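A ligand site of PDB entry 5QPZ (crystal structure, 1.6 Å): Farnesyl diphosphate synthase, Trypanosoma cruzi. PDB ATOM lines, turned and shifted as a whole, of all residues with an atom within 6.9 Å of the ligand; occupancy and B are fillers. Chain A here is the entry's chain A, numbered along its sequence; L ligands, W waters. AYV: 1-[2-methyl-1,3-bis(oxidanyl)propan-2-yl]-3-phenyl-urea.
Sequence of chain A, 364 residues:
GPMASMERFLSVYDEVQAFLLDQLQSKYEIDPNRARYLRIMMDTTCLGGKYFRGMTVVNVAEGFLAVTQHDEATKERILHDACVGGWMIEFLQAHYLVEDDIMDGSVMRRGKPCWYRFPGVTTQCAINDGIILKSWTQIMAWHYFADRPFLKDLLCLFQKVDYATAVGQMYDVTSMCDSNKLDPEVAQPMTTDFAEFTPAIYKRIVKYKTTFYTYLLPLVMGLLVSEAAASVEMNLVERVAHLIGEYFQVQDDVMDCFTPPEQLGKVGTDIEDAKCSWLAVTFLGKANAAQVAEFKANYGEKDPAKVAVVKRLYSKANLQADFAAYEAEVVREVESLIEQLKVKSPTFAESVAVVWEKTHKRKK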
ATOM      1  N   GLY A  48      19.664   0.214  14.210  1.00  0.00           N
ATOM      2  CA  GLY A  48      20.298   0.548  15.468  1.00  0.00           C
ATOM      3  C   GLY A  48      21.399   1.561  15.441  1.00  0.00           C
ATOM      4  O   GLY A  48      21.783   1.998  16.501  1.00  0.00           O
ATOM      5  N   GLY A  49      21.896   1.944  14.262  1.00  0.00           N
ATOM      6  CA  GLY A  49      22.722   3.131  14.090  1.00  0.00           C
ATOM      7  C   GLY A  49      21.912   4.479  14.098  1.00  0.00           C
ATOM      8  O   GLY A  49      20.762   4.498  14.480  1.00  0.00           O
ATOM      9  N   LYS A  50      22.535   5.583  13.655  1.00  0.00           N
ATOM     10  CA  LYS A  50      21.864   6.888  13.668  1.00  0.00           C
ATOM     11  C   LYS A  50      21.210   7.200  12.306  1.00  0.00           C
ATOM     12  O   LYS A  50      20.510   8.205  12.153  1.00  0.00           O
ATOM     13  CB  LYS A  50      22.874   7.959  14.082  1.00  0.00           C
ATOM     14  CG  LYS A  50      23.255   7.768  15.553  1.00  0.00           C
ATOM     15  CD  LYS A  50      24.440   8.583  16.011  1.00  0.00           C
ATOM     16  CE  LYS A  50      24.737   8.291  17.480  1.00  0.00           C
ATOM     17  NZ  LYS A  50      23.647   8.717  18.390  1.00  0.00           N
ATOM     18  N   TYR A  51      21.460   6.344  11.326  1.00  0.00           N
ATOM     19  CA  TYR A  51      20.814   6.458   9.974  1.00  0.00           C
ATOM     20  C   TYR A  51      21.265   7.761   9.375  1.00  0.00           C
ATOM     21  O   TYR A  51      20.557   8.363   8.479  1.00  0.00           O
ATOM     22  CB  TYR A  51      19.263   6.344   9.993  1.00  0.00           C
ATOM     23  CG  TYR A  51      18.798   5.126  10.794  1.00  0.00           C
ATOM     24  CD1 TYR A  51      19.161   3.853  10.390  1.00  0.00           C
ATOM     25  CD2 TYR A  51      18.057   5.287  11.960  1.00  0.00           C
ATOM     26  CE1 TYR A  51      18.769   2.744  11.126  1.00  0.00           C
ATOM     27  CE2 TYR A  51      17.639   4.197  12.698  1.00  0.00           C
ATOM     28  CZ  TYR A  51      18.023   2.928  12.321  1.00  0.00           C
ATOM     29  OH  TYR A  51      17.580   1.793  13.064  1.00  0.00           O
ATOM     30  N   PHE A  52      22.475   8.162   9.710  1.00  0.00           N
ATOM     31  CA  PHE A  52      23.042   9.338   9.058  1.00  0.00           C
ATOM     32  C   PHE A  52      23.005   9.318   7.526  1.00  0.00           C
ATOM     33  O   PHE A  52      22.568  10.319   6.910  1.00  0.00           O
ATOM     34  CB  PHE A  52      24.459   9.674   9.566  1.00  0.00           C
ATOM     35  CG  PHE A  52      25.169  10.706   8.775  1.00  0.00           C
ATOM     36  CD1 PHE A  52      24.897  12.006   9.019  1.00  0.00           C
ATOM     37  CD2 PHE A  52      26.099  10.370   7.770  1.00  0.00           C
ATOM     38  CE1 PHE A  52      25.557  12.964   8.278  1.00  0.00           C
ATOM     39  CE2 PHE A  52      26.732  11.352   7.009  1.00  0.00           C
ATOM     40  CZ  PHE A  52      26.460  12.633   7.284  1.00  0.00           C
ATOM     41  N   ARG A  53      23.503   8.260   6.936  1.00  0.00           N
ATOM     42  CA  ARG A  53      23.602   8.105   5.504  1.00  0.00           C
ATOM     43  C   ARG A  53      22.221   8.212   4.865  1.00  0.00           C
ATOM     44  O   ARG A  53      22.004   9.007   3.938  1.00  0.00           O
ATOM     45  CB  ARG A  53      24.371   6.885   5.141  1.00  0.00           C
ATOM     46  CG  ARG A  53      25.808   6.974   5.665  1.00  0.00           C
ATOM     47  CD  ARG A  53      26.493   5.655   5.542  1.00  0.00           C
ATOM     48  NE  ARG A  53      27.827   5.641   6.152  1.00  0.00           N
ATOM     49  CZ  ARG A  53      28.083   5.718   7.458  1.00  0.00           C
ATOM     50  NH1 ARG A  53      29.367   5.719   7.862  1.00  0.00           N
ATOM     51  NH2 ARG A  53      27.144   5.820   8.396  1.00  0.00           N
ATOM     52  N   ARG A 110      28.958  -1.599  17.556  1.00  0.00           N
ATOM     53  CA  ARG A 110      27.898  -0.778  18.156  1.00  0.00           C
ATOM     54  C   ARG A 110      27.252  -1.496  19.354  1.00  0.00           C
ATOM     55  O   ARG A 110      26.034  -1.639  19.468  1.00  0.00           O
ATOM     56  CB  ARG A 110      26.924  -0.326  17.045  1.00  0.00           C
ATOM     57  CG  ARG A 110      27.614   0.624  16.041  1.00  0.00           C
ATOM     58  CD  ARG A 110      27.051   0.613  14.616  1.00  0.00           C
ATOM     59  NE  ARG A 110      27.854   1.438  13.684  1.00  0.00           N
ATOM     60  CZ  ARG A 110      27.432   1.952  12.524  1.00  0.00           C
ATOM     61  NH1 ARG A 110      28.257   2.699  11.770  1.00  0.00           N
ATOM     62  NH2 ARG A 110      26.187   1.752  12.076  1.00  0.00           N
ATOM     63  N   THR A 214      29.642   7.146   2.450  1.00  0.00           N
ATOM     64  CA  THR A 214      29.144   7.801   3.591  1.00  0.00           C
ATOM     65  C   THR A 214      28.723   9.261   3.288  1.00  0.00           C
ATOM     66  O   THR A 214      27.800   9.751   3.943  1.00  0.00           O
ATOM     67  CB  THR A 214      30.214   7.836   4.693  1.00  0.00           C
ATOM     68  OG1 THR A 214      30.506   6.444   5.026  1.00  0.00           O
ATOM     69  CG2 THR A 214      29.776   8.605   5.932  1.00  0.00           C
ATOM     70  N   TYR A 215      29.460   9.905   2.426  1.00  0.00           N
ATOM     71  CA  TYR A 215      29.113  11.286   2.107  1.00  0.00           C
ATOM     72  C   TYR A 215      28.731  11.571   0.675  1.00  0.00           C
ATOM     73  O   TYR A 215      27.703  12.244   0.441  1.00  0.00           O
ATOM     74  CB  TYR A 215      30.300  12.188   2.500  1.00  0.00           C
ATOM     75  CG  TYR A 215      30.381  12.301   3.970  1.00  0.00           C
ATOM     76  CD1 TYR A 215      29.607  13.216   4.667  1.00  0.00           C
ATOM     77  CD2 TYR A 215      31.207  11.478   4.701  1.00  0.00           C
ATOM     78  CE1 TYR A 215      29.650  13.239   6.033  1.00  0.00           C
ATOM     79  CE2 TYR A 215      31.287  11.562   6.067  1.00  0.00           C
ATOM     80  CZ  TYR A 215      30.453  12.399   6.748  1.00  0.00           C
ATOM     81  OH  TYR A 215      30.505  12.502   8.124  1.00  0.00           O
ATOM     82  N   PHE A 248      35.679  12.738   9.139  1.00  0.00           N
ATOM     83  CA  PHE A 248      34.882  11.724   9.796  1.00  0.00           C
ATOM     84  C   PHE A 248      35.808  10.583  10.215  1.00  0.00           C
ATOM     85  O   PHE A 248      35.746  10.127  11.325  1.00  0.00           O
ATOM     86  CB  PHE A 248      33.865  11.182   8.803  1.00  0.00           C
ATOM     87  CG  PHE A 248      33.133   9.967   9.258  1.00  0.00           C
ATOM     88  CD1 PHE A 248      32.081  10.076  10.150  1.00  0.00           C
ATOM     89  CD2 PHE A 248      33.477   8.742   8.752  1.00  0.00           C
ATOM     90  CE1 PHE A 248      31.383   8.930  10.518  1.00  0.00           C
ATOM     91  CE2 PHE A 248      32.813   7.602   9.151  1.00  0.00           C
ATOM     92  CZ  PHE A 248      31.743   7.706  10.006  1.00  0.00           C
ATOM     93  N   GLN A 251      38.346  11.402  12.947  1.00  0.00           N
ATOM     94  CA  GLN A 251      37.634  11.272  14.186  1.00  0.00           C
ATOM     95  C   GLN A 251      37.502   9.835  14.628  1.00  0.00           C
ATOM     96  O   GLN A 251      37.697   9.540  15.802  1.00  0.00           O
ATOM     97  CB  GLN A 251      36.219  11.822  14.002  1.00  0.00           C
ATOM     98  CG  GLN A 251      36.040  13.311  13.963  1.00  0.00           C
ATOM     99  CD  GLN A 251      34.554  13.688  13.764  1.00  0.00           C
ATOM    100  OE1 GLN A 251      33.823  13.083  12.958  1.00  0.00           O
ATOM    101  NE2 GLN A 251      34.106  14.696  14.477  1.00  0.00           N
ATOM    102  N   ASP A 252      37.145   8.933  13.700  1.00  0.00           N
ATOM    103  CA  ASP A 252      37.006   7.515  14.013  1.00  0.00           C
ATOM    104  C   ASP A 252      38.346   6.910  14.437  1.00  0.00           C
ATOM    105  O   ASP A 252      38.380   6.103  15.360  1.00  0.00           O
ATOM    106  CB  ASP A 252      36.472   6.725  12.815  1.00  0.00           C
ATOM    107  CG  ASP A 252      36.511   5.204  13.031  1.00  0.00           C
ATOM    108  OD1 ASP A 252      35.701   4.663  13.845  1.00  0.00           O
ATOM    109  OD2 ASP A 252      37.352   4.543  12.397  1.00  0.00           O
ATOM    110  N   MET A 255      39.124   8.063  17.966  1.00  0.00           N
ATOM    111  CA  MET A 255      38.219   7.381  18.954  1.00  0.00           C
ATOM    112  C   MET A 255      38.662   5.923  19.233  1.00  0.00           C
ATOM    113  O   MET A 255      38.539   5.456  20.376  1.00  0.00           O
ATOM    114  CB  MET A 255      36.760   7.413  18.472  1.00  0.00           C
ATOM    115  CG  MET A 255      36.137   8.807  18.559  1.00  0.00           C
ATOM    116  SD  MET A 255      34.379   8.914  18.074  1.00  0.00           S
ATOM    117  CE  MET A 255      34.526   9.613  16.447  1.00  0.00           C
ATOM    118  N   GLN A 263      31.676   3.402  25.402  1.00  0.00           N
ATOM    119  CA  GLN A 263      31.243   4.544  24.572  1.00  0.00           C
ATOM    120  C   GLN A 263      31.481   4.266  23.105  1.00  0.00           C
ATOM    121  O   GLN A 263      30.626   4.514  22.249  1.00  0.00           O
ATOM    122  CB  GLN A 263      31.984   5.815  25.000  1.00  0.00           C
ATOM    123  CG  GLN A 263      31.494   7.075  24.305  1.00  0.00           C
ATOM    124  CD  GLN A 263      32.112   8.303  24.905  1.00  0.00           C
ATOM    125  OE1 GLN A 263      32.307   8.381  26.118  1.00  0.00           O
ATOM    126  NE2 GLN A 263      32.444   9.276  24.060  1.00  0.00           N
ATOM    127  N   LEU A 264      32.662   3.750  22.804  1.00  0.00           N
ATOM    128  CA  LEU A 264      32.993   3.317  21.435  1.00  0.00           C
ATOM    129  C   LEU A 264      32.043   2.217  20.820  1.00  0.00           C
ATOM    130  O   LEU A 264      31.870   2.193  19.633  1.00  0.00           O
ATOM    131  CB  LEU A 264      34.474   2.865  21.394  1.00  0.00           C
ATOM    132  CG  LEU A 264      35.159   2.565  20.058  1.00  0.00           C
ATOM    133  CD1 LEU A 264      35.095   3.737  19.081  1.00  0.00           C
ATOM    134  CD2 LEU A 264      36.611   2.211  20.330  1.00  0.00           C
ATOM    135  N   VAL A 355      25.040  18.497   7.152  1.00  0.00           N
ATOM    136  CA  VAL A 355      25.978  17.371   7.071  1.00  0.00           C
ATOM    137  C   VAL A 355      27.260  17.661   7.821  1.00  0.00           C
ATOM    138  O   VAL A 355      27.709  16.782   8.730  1.00  0.00           O
ATOM    139  CB  VAL A 355      26.209  17.016   5.635  1.00  0.00           C
ATOM    140  CG1 VAL A 355      27.443  16.147   5.501  1.00  0.00           C
ATOM    141  CG2 VAL A 355      24.989  16.290   5.057  1.00  0.00           C
ATOM    142  N   GLU A 357      27.680  20.002  10.258  1.00  0.00           N
ATOM    143  CA  GLU A 357      27.386  20.229  11.688  1.00  0.00           C
ATOM    144  C   GLU A 357      27.241  18.888  12.396  1.00  0.00           C
ATOM    145  O   GLU A 357      27.779  18.708  13.474  1.00  0.00           O
ATOM    146  CB  GLU A 357      26.101  21.065  11.923  1.00  0.00           C
ATOM    147  CG  GLU A 357      26.227  22.510  12.412  1.00  0.00           C
ATOM    148  CD  GLU A 357      24.991  23.368  11.980  1.00  0.00           C
ATOM    149  OE1 GLU A 357      23.849  22.965  12.338  1.00  0.00           O
ATOM    150  OE2 GLU A 357      25.156  24.403  11.259  1.00  0.00           O
ATOM    151  N   LYS A 358      26.510  17.962  11.791  1.00  0.00           N
ATOM    152  CA  LYS A 358      26.335  16.645  12.372  1.00  0.00           C
ATOM    153  C   LYS A 358      27.651  15.911  12.521  1.00  0.00           C
ATOM    154  O   LYS A 358      27.885  15.229  13.512  1.00  0.00           O
ATOM    155  CB  LYS A 358      25.375  15.836  11.544  1.00  0.00           C
ATOM    156  CG  LYS A 358      23.932  16.253  11.745  1.00  0.00           C
ATOM    157  CD  LYS A 358      23.065  15.437  10.788  1.00  0.00           C
ATOM    158  CE  LYS A 358      21.596  15.858  10.876  1.00  0.00           C
ATOM    159  NZ  LYS A 358      20.863  15.216   9.756  1.00  0.00           N
ATOM    160  N   THR A 359      28.530  16.014  11.546  1.00  0.00           N
ATOM    161  CA  THR A 359      29.852  15.354  11.620  1.00  0.00           C
ATOM    162  C   THR A 359      30.803  15.963  12.653  1.00  0.00           C
ATOM    163  O   THR A 359      31.452  15.247  13.451  1.00  0.00           O
ATOM    164  CB  THR A 359      30.550  15.439  10.274  1.00  0.00           C
ATOM    165  OG1 THR A 359      29.744  14.818   9.256  1.00  0.00           O
ATOM    166  CG2 THR A 359      31.920  14.753  10.302  1.00  0.00           C
ATOM    167  N   HIS A 360      30.848  17.287  12.659  1.00  0.00           N
ATOM    168  CA  HIS A 360      31.717  18.104  13.533  1.00  0.00           C
ATOM    169  C   HIS A 360      31.430  17.922  15.012  1.00  0.00           C
ATOM    170  O   HIS A 360      32.330  18.087  15.793  1.00  0.00           O
ATOM    171  CB  HIS A 360      31.533  19.576  13.157  1.00  0.00           C
ATOM    172  CG  HIS A 360      32.540  20.515  13.733  1.00  0.00           C
ATOM    173  ND1 HIS A 360      32.238  21.821  13.998  1.00  0.00           N
ATOM    174  CD2 HIS A 360      33.851  20.349  14.048  1.00  0.00           C
ATOM    175  CE1 HIS A 360      33.320  22.432  14.464  1.00  0.00           C
ATOM    176  NE2 HIS A 360      34.307  21.563  14.503  1.00  0.00           N
ATOM    177  N   LYS A 361      30.223  17.514  15.392  1.00  0.00           N
ATOM    178  CA  LYS A 361      29.864  17.262  16.799  1.00  0.00           C
ATOM    179  C   LYS A 361      29.426  15.798  17.009  1.00  0.00           C
ATOM    180  O   LYS A 361      28.238  15.489  16.951  1.00  0.00           O
ATOM    181  CB  LYS A 361      28.804  18.277  17.318  1.00  0.00           C
ATOM    182  CG  LYS A 361      27.794  18.817  16.287  1.00  0.00           C
ATOM    183  CD  LYS A 361      26.360  18.955  16.764  1.00  0.00           C
ATOM    184  CE  LYS A 361      25.592  17.618  16.645  1.00  0.00           C
ATOM    185  NZ  LYS A 361      24.641  17.361  17.771  1.00  0.00           N
ATOM    186  N   ARG A 362      30.402  14.912  17.235  1.00  0.00           N
ATOM    187  CA  ARG A 362      30.163  13.517  17.621  1.00  0.00           C
ATOM    188  C   ARG A 362      31.392  12.936  18.345  1.00  0.00           C
ATOM    189  O   ARG A 362      31.453  12.895  19.583  1.00  0.00           O
ATOM    190  CB  ARG A 362      29.781  12.669  16.389  1.00  0.00           C
ATOM    191  CG  ARG A 362      30.918  12.358  15.426  1.00  0.00           C
ATOM    192  CD  ARG A 362      30.473  11.657  14.148  1.00  0.00           C
ATOM    193  NE  ARG A 362      31.637  11.063  13.477  1.00  0.00           N
ATOM    194  CZ  ARG A 362      32.111   9.820  13.642  1.00  0.00           C
ATOM    195  NH1 ARG A 362      31.517   8.938  14.453  1.00  0.00           N
ATOM    196  NH2 ARG A 362      33.207   9.441  12.984  1.00  0.00           N
HETATM  197  N1  AYV L   1      27.542   6.525  14.318  1.00  0.00           N
HETATM  198  C4  AYV L   1      28.043   4.226  15.024  1.00  0.00           C
HETATM  199  C5  AYV L   1      27.801   7.838  13.952  1.00  0.00           C
HETATM  200  C6  AYV L   1      27.404   9.570  12.135  1.00  0.00           C
HETATM  201  C7  AYV L   1      27.008  10.752  12.805  1.00  0.00           C
HETATM  202  C8  AYV L   1      27.324  11.986  12.240  1.00  0.00           C
HETATM  203  C10 AYV L   1      28.385  10.902  10.349  1.00  0.00           C
HETATM  204  C1  AYV L   1      27.579   5.999  16.794  1.00  0.00           C
HETATM  205  C2  AYV L   1      28.201   5.731  15.405  1.00  0.00           C
HETATM  206  C3  AYV L   1      29.724   6.010  15.550  1.00  0.00           C
HETATM  207  O1  AYV L   1      30.363   5.757  14.344  1.00  0.00           O
HETATM  208  O2  AYV L   1      26.679   3.963  14.960  1.00  0.00           O
HETATM  209  O3  AYV L   1      28.452   8.618  14.631  1.00  0.00           O
HETATM  210  N2  AYV L   1      27.235   8.252  12.698  1.00  0.00           N
HETATM  211  C9  AYV L   1      28.014  12.065  11.017  1.00  0.00           C
HETATM  212  C11 AYV L   1      28.067   9.652  10.883  1.00  0.00           C
HETATM  213  O   HOH W   1      26.627  10.746  16.410  1.00  0.00           O
HETATM  214  O   HOH W   2      31.563   5.026  12.390  1.00  0.00           O
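Lys 50 touches the ligand (CE to C1, 3.7 Å).
Phe 52 touches the ligand (CD2 to C10, 3.5 Å).
Tyr 215 touches the ligand.
CE1 of Phe 248 touches C11 of the ligand, at 3.4 Å.
Lys 358 touches the ligand (O to C8, 3.5 Å).
Thr 359 touches the ligand (OG1 to C9, 3.7 Å).
Hydrophobic or aromatic side chains that line the ligand: Phe 52 and Phe 248.
Eight residues have an atom within 4 Å of the ligand: Lys 50, Phe 52, Arg 110, Tyr 215, Phe 248, Lys 358, Thr 359 and Arg 362.
The nearest printed residue that does not touch the ligand is Gly 49 (4.1 Å).
The guanidinium group (NH2) of Arg 362 is in hydrogen-bond range of the backbone carbonyl oxygen (O) of Phe 248, at 3.1 Å.
OG1 of Thr 359 lies within hydrogen-bond range of O of Val 355 (2.9 Å).
The backbone carbonyl oxygen (O) of Thr 359 lies within hydrogen-bond range of the side-chain amide nitrogen (NE2) of Gln 251, 2.9 Å away.
The side-chain amide oxygen (OE1) of Gln 251 sits at hydrogen-bond distance from the guanidinium group (NE) of Arg 362, at 3.0 Å.
The side-chain hydroxyl (OH) of Tyr 215 lies within hydrogen-bond range of the side-chain hydroxyl (OG1) of Thr 359, at 2.7 Å.
The guanidinium group (NH1) of Arg 362 lies within hydrogen-bond range of an oxygen (O3) of the ligand, 3.1 Å away.
The guanidinium group (NE) of Arg 110 sits at hydrogen-bond distance from an oxygen (O2) of the ligand (3.1 Å).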
